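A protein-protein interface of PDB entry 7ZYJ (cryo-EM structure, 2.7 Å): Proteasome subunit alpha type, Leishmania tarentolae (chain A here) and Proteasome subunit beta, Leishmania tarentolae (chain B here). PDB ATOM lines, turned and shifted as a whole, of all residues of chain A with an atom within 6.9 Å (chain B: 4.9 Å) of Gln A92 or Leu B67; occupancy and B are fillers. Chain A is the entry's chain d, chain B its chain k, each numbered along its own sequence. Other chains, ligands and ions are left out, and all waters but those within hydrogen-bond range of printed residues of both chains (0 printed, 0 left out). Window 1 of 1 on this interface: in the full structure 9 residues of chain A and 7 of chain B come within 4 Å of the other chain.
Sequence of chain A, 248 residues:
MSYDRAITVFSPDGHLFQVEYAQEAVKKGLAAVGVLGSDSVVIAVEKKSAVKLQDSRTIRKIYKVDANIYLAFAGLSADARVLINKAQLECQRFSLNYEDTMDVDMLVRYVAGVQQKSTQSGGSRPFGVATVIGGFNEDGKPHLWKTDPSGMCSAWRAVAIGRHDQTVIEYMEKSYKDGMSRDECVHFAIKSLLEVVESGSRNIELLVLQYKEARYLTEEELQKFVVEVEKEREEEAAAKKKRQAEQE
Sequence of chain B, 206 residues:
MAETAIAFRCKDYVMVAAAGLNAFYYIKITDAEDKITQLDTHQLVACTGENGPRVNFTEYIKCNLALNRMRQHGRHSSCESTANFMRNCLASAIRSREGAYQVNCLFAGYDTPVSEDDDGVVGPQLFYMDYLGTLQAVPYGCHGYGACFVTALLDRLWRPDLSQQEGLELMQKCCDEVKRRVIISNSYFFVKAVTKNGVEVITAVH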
ATOM      1  N   VAL A  65      11.855  17.791 -12.474  1.00  0.00           N
ATOM      2  CA  VAL A  65      13.127  17.561 -11.801  1.00  0.00           C
ATOM      3  C   VAL A  65      13.511  16.089 -11.877  1.00  0.00           C
ATOM      4  O   VAL A  65      14.681  15.750 -12.088  1.00  0.00           O
ATOM      5  CB  VAL A  65      13.063  18.055 -10.348  1.00  0.00           C
ATOM      6  CG1 VAL A  65      14.364  17.742  -9.639  1.00  0.00           C
ATOM      7  CG2 VAL A  65      12.775  19.546 -10.307  1.00  0.00           C
ATOM      8  N   ASP A  66      12.540  15.196 -11.718  1.00  0.00           N
ATOM      9  CA  ASP A  66      12.783  13.766 -11.834  1.00  0.00           C
ATOM     10  C   ASP A  66      11.494  13.108 -12.300  1.00  0.00           C
ATOM     11  O   ASP A  66      10.424  13.722 -12.293  1.00  0.00           O
ATOM     12  CB  ASP A  66      13.266  13.168 -10.509  1.00  0.00           C
ATOM     13  CG  ASP A  66      14.142  11.948 -10.708  1.00  0.00           C
ATOM     14  OD1 ASP A  66      14.276  11.497 -11.865  1.00  0.00           O
ATOM     15  OD2 ASP A  66      14.696  11.442  -9.711  1.00  0.00           O
ATOM     16  N   ALA A  67      11.609  11.833 -12.682  1.00  0.00           N
ATOM     17  CA  ALA A  67      10.479  11.117 -13.267  1.00  0.00           C
ATOM     18  C   ALA A  67       9.257  11.145 -12.363  1.00  0.00           C
ATOM     19  O   ALA A  67       8.121  11.104 -12.851  1.00  0.00           O
ATOM     20  CB  ALA A  67      10.876   9.672 -13.572  1.00  0.00           C
ATOM     21  N   ASN A  85      18.390  22.942 -12.032  1.00  0.00           N
ATOM     22  CA  ASN A  85      19.524  22.143 -12.485  1.00  0.00           C
ATOM     23  C   ASN A  85      20.224  21.477 -11.308  1.00  0.00           C
ATOM     24  O   ASN A  85      20.605  20.301 -11.384  1.00  0.00           O
ATOM     25  CB  ASN A  85      20.501  23.015 -13.270  1.00  0.00           C
ATOM     26  CG  ASN A  85      19.990  23.360 -14.653  1.00  0.00           C
ATOM     27  OD1 ASN A  85      19.112  22.686 -15.187  1.00  0.00           O
ATOM     28  ND2 ASN A  85      20.539  24.417 -15.239  1.00  0.00           N
ATOM     29  N   ALA A  87      18.806  20.647  -8.475  1.00  0.00           N
ATOM     30  CA  ALA A  87      17.918  19.597  -7.986  1.00  0.00           C
ATOM     31  C   ALA A  87      17.977  18.357  -8.872  1.00  0.00           C
ATOM     32  O   ALA A  87      17.970  17.227  -8.372  1.00  0.00           O
ATOM     33  CB  ALA A  87      16.488  20.124  -7.892  1.00  0.00           C
ATOM     34  N   GLN A  88      18.023  18.547 -10.191  1.00  0.00           N
ATOM     35  CA  GLN A  88      18.124  17.413 -11.106  1.00  0.00           C
ATOM     36  C   GLN A  88      19.444  16.675 -10.920  1.00  0.00           C
ATOM     37  O   GLN A  88      19.482  15.435 -10.900  1.00  0.00           O
ATOM     38  CB  GLN A  88      17.970  17.893 -12.549  1.00  0.00           C
ATOM     39  CG  GLN A  88      16.582  18.409 -12.881  1.00  0.00           C
ATOM     40  CD  GLN A  88      16.547  19.206 -14.168  1.00  0.00           C
ATOM     41  OE1 GLN A  88      17.556  19.770 -14.589  1.00  0.00           O
ATOM     42  NE2 GLN A  88      15.382  19.260 -14.799  1.00  0.00           N
ATOM     43  N   LEU A  89      20.542  17.423 -10.782  1.00  0.00           N
ATOM     44  CA  LEU A  89      21.830  16.792 -10.521  1.00  0.00           C
ATOM     45  C   LEU A  89      21.819  16.035  -9.202  1.00  0.00           C
ATOM     46  O   LEU A  89      22.396  14.948  -9.107  1.00  0.00           O
ATOM     47  CB  LEU A  89      22.939  17.844 -10.527  1.00  0.00           C
ATOM     48  CG  LEU A  89      24.362  17.331 -10.304  1.00  0.00           C
ATOM     49  CD1 LEU A  89      24.930  16.766 -11.593  1.00  0.00           C
ATOM     50  CD2 LEU A  89      25.255  18.436  -9.765  1.00  0.00           C
ATOM     51  N   GLU A  90      21.162  16.587  -8.178  1.00  0.00           N
ATOM     52  CA  GLU A  90      21.060  15.893  -6.900  1.00  0.00           C
ATOM     53  C   GLU A  90      20.251  14.611  -7.023  1.00  0.00           C
ATOM     54  O   GLU A  90      20.608  13.589  -6.429  1.00  0.00           O
ATOM     55  CB  GLU A  90      20.438  16.811  -5.851  1.00  0.00           C
ATOM     56  CG  GLU A  90      20.308  16.182  -4.475  1.00  0.00           C
ATOM     57  CD  GLU A  90      21.610  15.585  -3.976  1.00  0.00           C
ATOM     58  OE1 GLU A  90      22.670  16.217  -4.164  1.00  0.00           O
ATOM     59  OE2 GLU A  90      21.571  14.482  -3.392  1.00  0.00           O
ATOM     60  N   CYS A  91      19.150  14.647  -7.777  1.00  0.00           N
ATOM     61  CA  CYS A  91      18.358  13.437  -7.977  1.00  0.00           C
ATOM     62  C   CYS A  91      19.173  12.359  -8.677  1.00  0.00           C
ATOM     63  O   CYS A  91      19.138  11.185  -8.285  1.00  0.00           O
ATOM     64  CB  CYS A  91      17.096  13.755  -8.778  1.00  0.00           C
ATOM     65  SG  CYS A  91      15.758  14.494  -7.821  1.00  0.00           S
ATOM     66  N   GLN A  92      19.921  12.740  -9.716  1.00  0.00           N
ATOM     67  CA  GLN A  92      20.745  11.758 -10.414  1.00  0.00           C
ATOM     68  C   GLN A  92      21.858  11.218  -9.523  1.00  0.00           C
ATOM     69  O   GLN A  92      22.127  10.012  -9.533  1.00  0.00           O
ATOM     70  CB  GLN A  92      21.323  12.365 -11.688  1.00  0.00           C
ATOM     71  CG  GLN A  92      20.277  12.649 -12.750  1.00  0.00           C
ATOM     72  CD  GLN A  92      19.378  11.457 -13.025  1.00  0.00           C
ATOM     73  OE1 GLN A  92      19.847  10.328 -13.162  1.00  0.00           O
ATOM     74  NE2 GLN A  92      18.077  11.705 -13.105  1.00  0.00           N
ATOM     75  N   ARG A  93      22.504  12.084  -8.740  1.00  0.00           N
ATOM     76  CA  ARG A  93      23.543  11.625  -7.826  1.00  0.00           C
ATOM     77  C   ARG A  93      22.974  10.684  -6.772  1.00  0.00           C
ATOM     78  O   ARG A  93      23.618   9.696  -6.400  1.00  0.00           O
ATOM     79  CB  ARG A  93      24.225  12.825  -7.170  1.00  0.00           C
ATOM     80  CG  ARG A  93      25.437  12.477  -6.327  1.00  0.00           C
ATOM     81  CD  ARG A  93      25.561  13.416  -5.144  1.00  0.00           C
ATOM     82  NE  ARG A  93      24.375  13.384  -4.298  1.00  0.00           N
ATOM     83  CZ  ARG A  93      24.222  12.584  -3.252  1.00  0.00           C
ATOM     84  NH1 ARG A  93      25.169  11.736  -2.886  1.00  0.00           N
ATOM     85  NH2 ARG A  93      23.090  12.635  -2.556  1.00  0.00           N
ATOM     86  N   PHE A  94      21.771  10.976  -6.277  1.00  0.00           N
ATOM     87  CA  PHE A  94      21.117  10.101  -5.314  1.00  0.00           C
ATOM     88  C   PHE A  94      20.829   8.737  -5.927  1.00  0.00           C
ATOM     89  O   PHE A  94      21.126   7.697  -5.331  1.00  0.00           O
ATOM     90  CB  PHE A  94      19.830  10.757  -4.813  1.00  0.00           C
ATOM     91  CG  PHE A  94      19.160  10.012  -3.696  1.00  0.00           C
ATOM     92  CD1 PHE A  94      18.327   8.938  -3.958  1.00  0.00           C
ATOM     93  CD2 PHE A  94      19.358  10.393  -2.381  1.00  0.00           C
ATOM     94  CE1 PHE A  94      17.712   8.256  -2.932  1.00  0.00           C
ATOM     95  CE2 PHE A  94      18.742   9.714  -1.352  1.00  0.00           C
ATOM     96  CZ  PHE A  94      17.917   8.647  -1.630  1.00  0.00           C
ATOM     97  N   SER A  95      20.251   8.722  -7.128  1.00  0.00           N
ATOM     98  CA  SER A  95      19.919   7.464  -7.795  1.00  0.00           C
ATOM     99  C   SER A  95      21.152   6.736  -8.311  1.00  0.00           C
ATOM    100  O   SER A  95      21.070   5.586  -8.744  1.00  0.00           O
ATOM    101  CB  SER A  95      18.933   7.732  -8.928  1.00  0.00           C
ATOM    102  OG  SER A  95      19.570   8.386 -10.013  1.00  0.00           O
ATOM    103  N   LEU A  96      22.309   7.396  -8.278  1.00  0.00           N
ATOM    104  CA  LEU A  96      23.570   6.739  -8.605  1.00  0.00           C
ATOM    105  C   LEU A  96      24.356   6.275  -7.388  1.00  0.00           C
ATOM    106  O   LEU A  96      25.171   5.356  -7.523  1.00  0.00           O
ATOM    107  CB  LEU A  96      24.449   7.678  -9.442  1.00  0.00           C
ATOM    108  CG  LEU A  96      25.809   7.197  -9.948  1.00  0.00           C
ATOM    109  CD1 LEU A  96      25.636   6.023 -10.890  1.00  0.00           C
ATOM    110  CD2 LEU A  96      26.543   8.331 -10.637  1.00  0.00           C
ATOM    111  N   ASN A  97      24.135   6.845  -6.204  1.00  0.00           N
ATOM    112  CA  ASN A  97      24.835   6.416  -5.002  1.00  0.00           C
ATOM    113  C   ASN A  97      24.036   5.432  -4.159  1.00  0.00           C
ATOM    114  O   ASN A  97      24.616   4.776  -3.287  1.00  0.00           O
ATOM    115  CB  ASN A  97      25.204   7.628  -4.140  1.00  0.00           C
ATOM    116  CG  ASN A  97      26.195   8.548  -4.822  1.00  0.00           C
ATOM    117  OD1 ASN A  97      26.217   9.752  -4.569  1.00  0.00           O
ATOM    118  ND2 ASN A  97      27.025   7.985  -5.691  1.00  0.00           N
ATOM    119  N   MET A 102      15.133   9.204  -5.461  1.00  0.00           N
ATOM    120  CA  MET A 102      15.009  10.146  -4.359  1.00  0.00           C
ATOM    121  C   MET A 102      13.544  10.375  -4.012  1.00  0.00           C
ATOM    122  O   MET A 102      12.702  10.567  -4.893  1.00  0.00           O
ATOM    123  CB  MET A 102      15.673  11.473  -4.725  1.00  0.00           C
ATOM    124  CG  MET A 102      16.087  12.321  -3.538  1.00  0.00           C
ATOM    125  SD  MET A 102      17.373  13.506  -3.970  1.00  0.00           S
ATOM    126  CE  MET A 102      17.933  14.006  -2.346  1.00  0.00           C
ATOM    127  N   CYS B  63      22.676   7.130 -15.761  1.00  0.00           N
ATOM    128  CA  CYS B  63      22.330   8.321 -14.996  1.00  0.00           C
ATOM    129  C   CYS B  63      22.630   9.587 -15.782  1.00  0.00           C
ATOM    130  O   CYS B  63      21.855  10.548 -15.739  1.00  0.00           O
ATOM    131  CB  CYS B  63      23.079   8.322 -13.663  1.00  0.00           C
ATOM    132  SG  CYS B  63      22.327   7.276 -12.397  1.00  0.00           S
ATOM    133  N   ASN B  64      23.750   9.613 -16.510  1.00  0.00           N
ATOM    134  CA  ASN B  64      24.059  10.788 -17.317  1.00  0.00           C
ATOM    135  C   ASN B  64      23.058  10.961 -18.453  1.00  0.00           C
ATOM    136  O   ASN B  64      22.656  12.089 -18.763  1.00  0.00           O
ATOM    137  CB  ASN B  64      25.483  10.697 -17.856  1.00  0.00           C
ATOM    138  CG  ASN B  64      26.516  11.103 -16.827  1.00  0.00           C
ATOM    139  OD1 ASN B  64      27.049  12.209 -16.870  1.00  0.00           O
ATOM    140  ND2 ASN B  64      26.796  10.209 -15.887  1.00  0.00           N
ATOM    141  N   LEU B  65      22.637   9.860 -19.080  1.00  0.00           N
ATOM    142  CA  LEU B  65      21.614   9.956 -20.117  1.00  0.00           C
ATOM    143  C   LEU B  65      20.302  10.479 -19.548  1.00  0.00           C
ATOM    144  O   LEU B  65      19.640  11.324 -20.166  1.00  0.00           O
ATOM    145  CB  LEU B  65      21.401   8.595 -20.778  1.00  0.00           C
ATOM    146  CG  LEU B  65      22.546   8.041 -21.622  1.00  0.00           C
ATOM    147  CD1 LEU B  65      22.227   6.621 -22.048  1.00  0.00           C
ATOM    148  CD2 LEU B  65      22.803   8.928 -22.827  1.00  0.00           C
ATOM    149  N   ALA B  66      19.906   9.986 -18.373  1.00  0.00           N
ATOM    150  CA  ALA B  66      18.679  10.465 -17.746  1.00  0.00           C
ATOM    151  C   ALA B  66      18.779  11.944 -17.396  1.00  0.00           C
ATOM    152  O   ALA B  66      17.819  12.701 -17.583  1.00  0.00           O
ATOM    153  CB  ALA B  66      18.368   9.636 -16.500  1.00  0.00           C
ATOM    154  N   LEU B  67      19.934  12.375 -16.884  1.00  0.00           N
ATOM    155  CA  LEU B  67      20.120  13.784 -16.555  1.00  0.00           C
ATOM    156  C   LEU B  67      20.054  14.653 -17.802  1.00  0.00           C
ATOM    157  O   LEU B  67      19.472  15.745 -17.775  1.00  0.00           O
ATOM    158  CB  LEU B  67      21.450  13.981 -15.830  1.00  0.00           C
ATOM    159  CG  LEU B  67      21.772  15.396 -15.351  1.00  0.00           C
ATOM    160  CD1 LEU B  67      20.572  16.016 -14.656  1.00  0.00           C
ATOM    161  CD2 LEU B  67      22.973  15.376 -14.424  1.00  0.00           C
ATOM    162  N   ASN B  68      20.654  14.194 -18.902  1.00  0.00           N
ATOM    163  CA  ASN B  68      20.563  14.938 -20.154  1.00  0.00           C
ATOM    164  C   ASN B  68      19.120  15.030 -20.631  1.00  0.00           C
ATOM    165  O   ASN B  68      18.677  16.090 -21.085  1.00  0.00           O
ATOM    166  CB  ASN B  68      21.442  14.290 -21.220  1.00  0.00           C
ATOM    167  CG  ASN B  68      22.915  14.356 -20.877  1.00  0.00           C
ATOM    168  OD1 ASN B  68      23.296  14.871 -19.828  1.00  0.00           O
ATOM    169  ND2 ASN B  68      23.752  13.834 -21.763  1.00  0.00           N
ATOM    170  N   ARG B  69      18.368  13.933 -20.529  1.00  0.00           N
ATOM    171  CA  ARG B  69      16.959  13.974 -20.912  1.00  0.00           C
ATOM    172  C   ARG B  69      16.180  14.955 -20.045  1.00  0.00           C
ATOM    173  O   ARG B  69      15.288  15.656 -20.536  1.00  0.00           O
ATOM    174  CB  ARG B  69      16.347  12.577 -20.828  1.00  0.00           C
ATOM    175  CG  ARG B  69      16.559  11.734 -22.071  1.00  0.00           C
ATOM    176  CD  ARG B  69      15.530  10.617 -22.165  1.00  0.00           C
ATOM    177  NE  ARG B  69      15.320   9.939 -20.890  1.00  0.00           N
ATOM    178  CZ  ARG B  69      16.195   9.126 -20.313  1.00  0.00           C
ATOM    179  NH1 ARG B  69      17.358   8.846 -20.878  1.00  0.00           N
ATOM    180  NH2 ARG B  69      15.891   8.573 -19.142  1.00  0.00           N
ATOM    181  N   MET B  70      16.496  15.011 -18.750  1.00  0.00           N
ATOM    182  CA  MET B  70      15.842  15.970 -17.866  1.00  0.00           C
ATOM    183  C   MET B  70      16.162  17.403 -18.277  1.00  0.00           C
ATOM    184  O   MET B  70      15.265  18.245 -18.402  1.00  0.00           O
ATOM    185  CB  MET B  70      16.261  15.724 -16.414  1.00  0.00           C
ATOM    186  CG  MET B  70      15.809  14.392 -15.848  1.00  0.00           C
ATOM    187  SD  MET B  70      14.018  14.239 -15.750  1.00  0.00           S
ATOM    188  CE  MET B  70      13.863  12.517 -15.285  1.00  0.00           C
ATOM    189  N   ARG B  71      17.443  17.698 -18.499  1.00  0.00           N
ATOM    190  CA  ARG B  71      17.856  19.053 -18.844  1.00  0.00           C
ATOM    191  C   ARG B  71      17.542  19.427 -20.285  1.00  0.00           C
ATOM    192  O   ARG B  71      17.695  20.601 -20.643  1.00  0.00           O
ATOM    193  CB  ARG B  71      19.350  19.234 -18.579  1.00  0.00           C
ATOM    194  CG  ARG B  71      19.689  19.489 -17.121  1.00  0.00           C
ATOM    195  CD  ARG B  71      21.103  19.053 -16.791  1.00  0.00           C
ATOM    196  NE  ARG B  71      21.422  19.273 -15.385  1.00  0.00           N
ATOM    197  CZ  ARG B  71      22.633  19.135 -14.862  1.00  0.00           C
ATOM    198  NH1 ARG B  71      23.668  18.771 -15.601  1.00  0.00           N
ATOM    199  NH2 ARG B  71      22.808  19.368 -13.564  1.00  0.00           N
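SG of Cys A91 lies close to OD2 of Asp A66 (3.7 Å). The side-chain amide oxygen (OD1) of Asn A85 sits close to the side-chain amide oxygen (OE1) of Gln A88 (3.4 Å). O of Cys A91 sits at hydrogen-bond distance from OG of Ser A95, at 3.3 Å. The backbone carbonyl oxygen of Gln A92 sits at hydrogen-bond distance from the side-chain hydroxyl of Ser A95 (3.1 Å).
The backbone carbonyl oxygen of Cys B63 lies close to the side-chain amide oxygen of Gln A92 (3.3 Å). The guanidinium group (NH2) of Arg B71 sits at hydrogen-bond distance from the backbone carbonyl oxygen (O) of Asn A85 (3.2 Å).
Of the printed residues of chain B, Asp A66 touches Met B70 (3.6 Å). Of the printed residues of chain B, Asn A85 touches Arg B71. Of chain B, only Cys B63 (3.3 Å), Ala B66 (3.7 Å) and Leu B67 (3.6 Å) come within 4 Å of Gln A92. Of the printed residues of chain B, Ser A95 touches Cys B63 (3.8 Å). Of the printed residues of chain B, Leu A96 touches Cys B63 (3.7 Å). Of the printed residues of chain A, Leu B67 touches Gln A88, Leu A89 and Gln A92. Printed residues of chain A within 4 Å of Arg B71: Asn A85, Gln A88 and Leu A89. The nearest residue of chain B that does not touch Gln A92 is Met B70 (4.5 Å).
Of the 9 printed residues of chain B, 5 touch a printed residue of chain A. Hydrophobic or aromatic side chains of chain B within 4 Å of the printed part of chain A: Ala B66, Leu B67 and Met B70. Printed residues of chain A that touch a printed residue of chain B: Asp A66, Ala A67, Asn A85, Gln A88, Leu A89, Gln A92, Ser A95 and Leu A96. Hydrophobic or aromatic side chains of chain A that line the printed part of chain B: Leu A89 and Leu A96. Among the printed residues, 13 pairs touch across the chains. Among the printed residues, no Asp or Glu carboxylate lies within 4 Å of a Lys or Arg side-chain nitrogen of the other chain.
Asp A66 touches Met B70 (OD1 to CE, 3.6 Å). Ala A67 touches Met B70. Gln A88 touches Leu B67 (CB to CD1, 3.8 Å). Gln A88 touches Met B70 (NE2 to O, 3.7 Å). OE1 of Gln A88 touches CG of Arg B71 (3.3 Å). Leu A89 touches Arg B71 (CB to NH2, 3.4 Å). Gln A92 touches Ala B66. Gln A92 touches Leu B67 (CG to CB, 3.6 Å). Ser A95 touches Cys B63. Leu A96 touches Cys B63.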
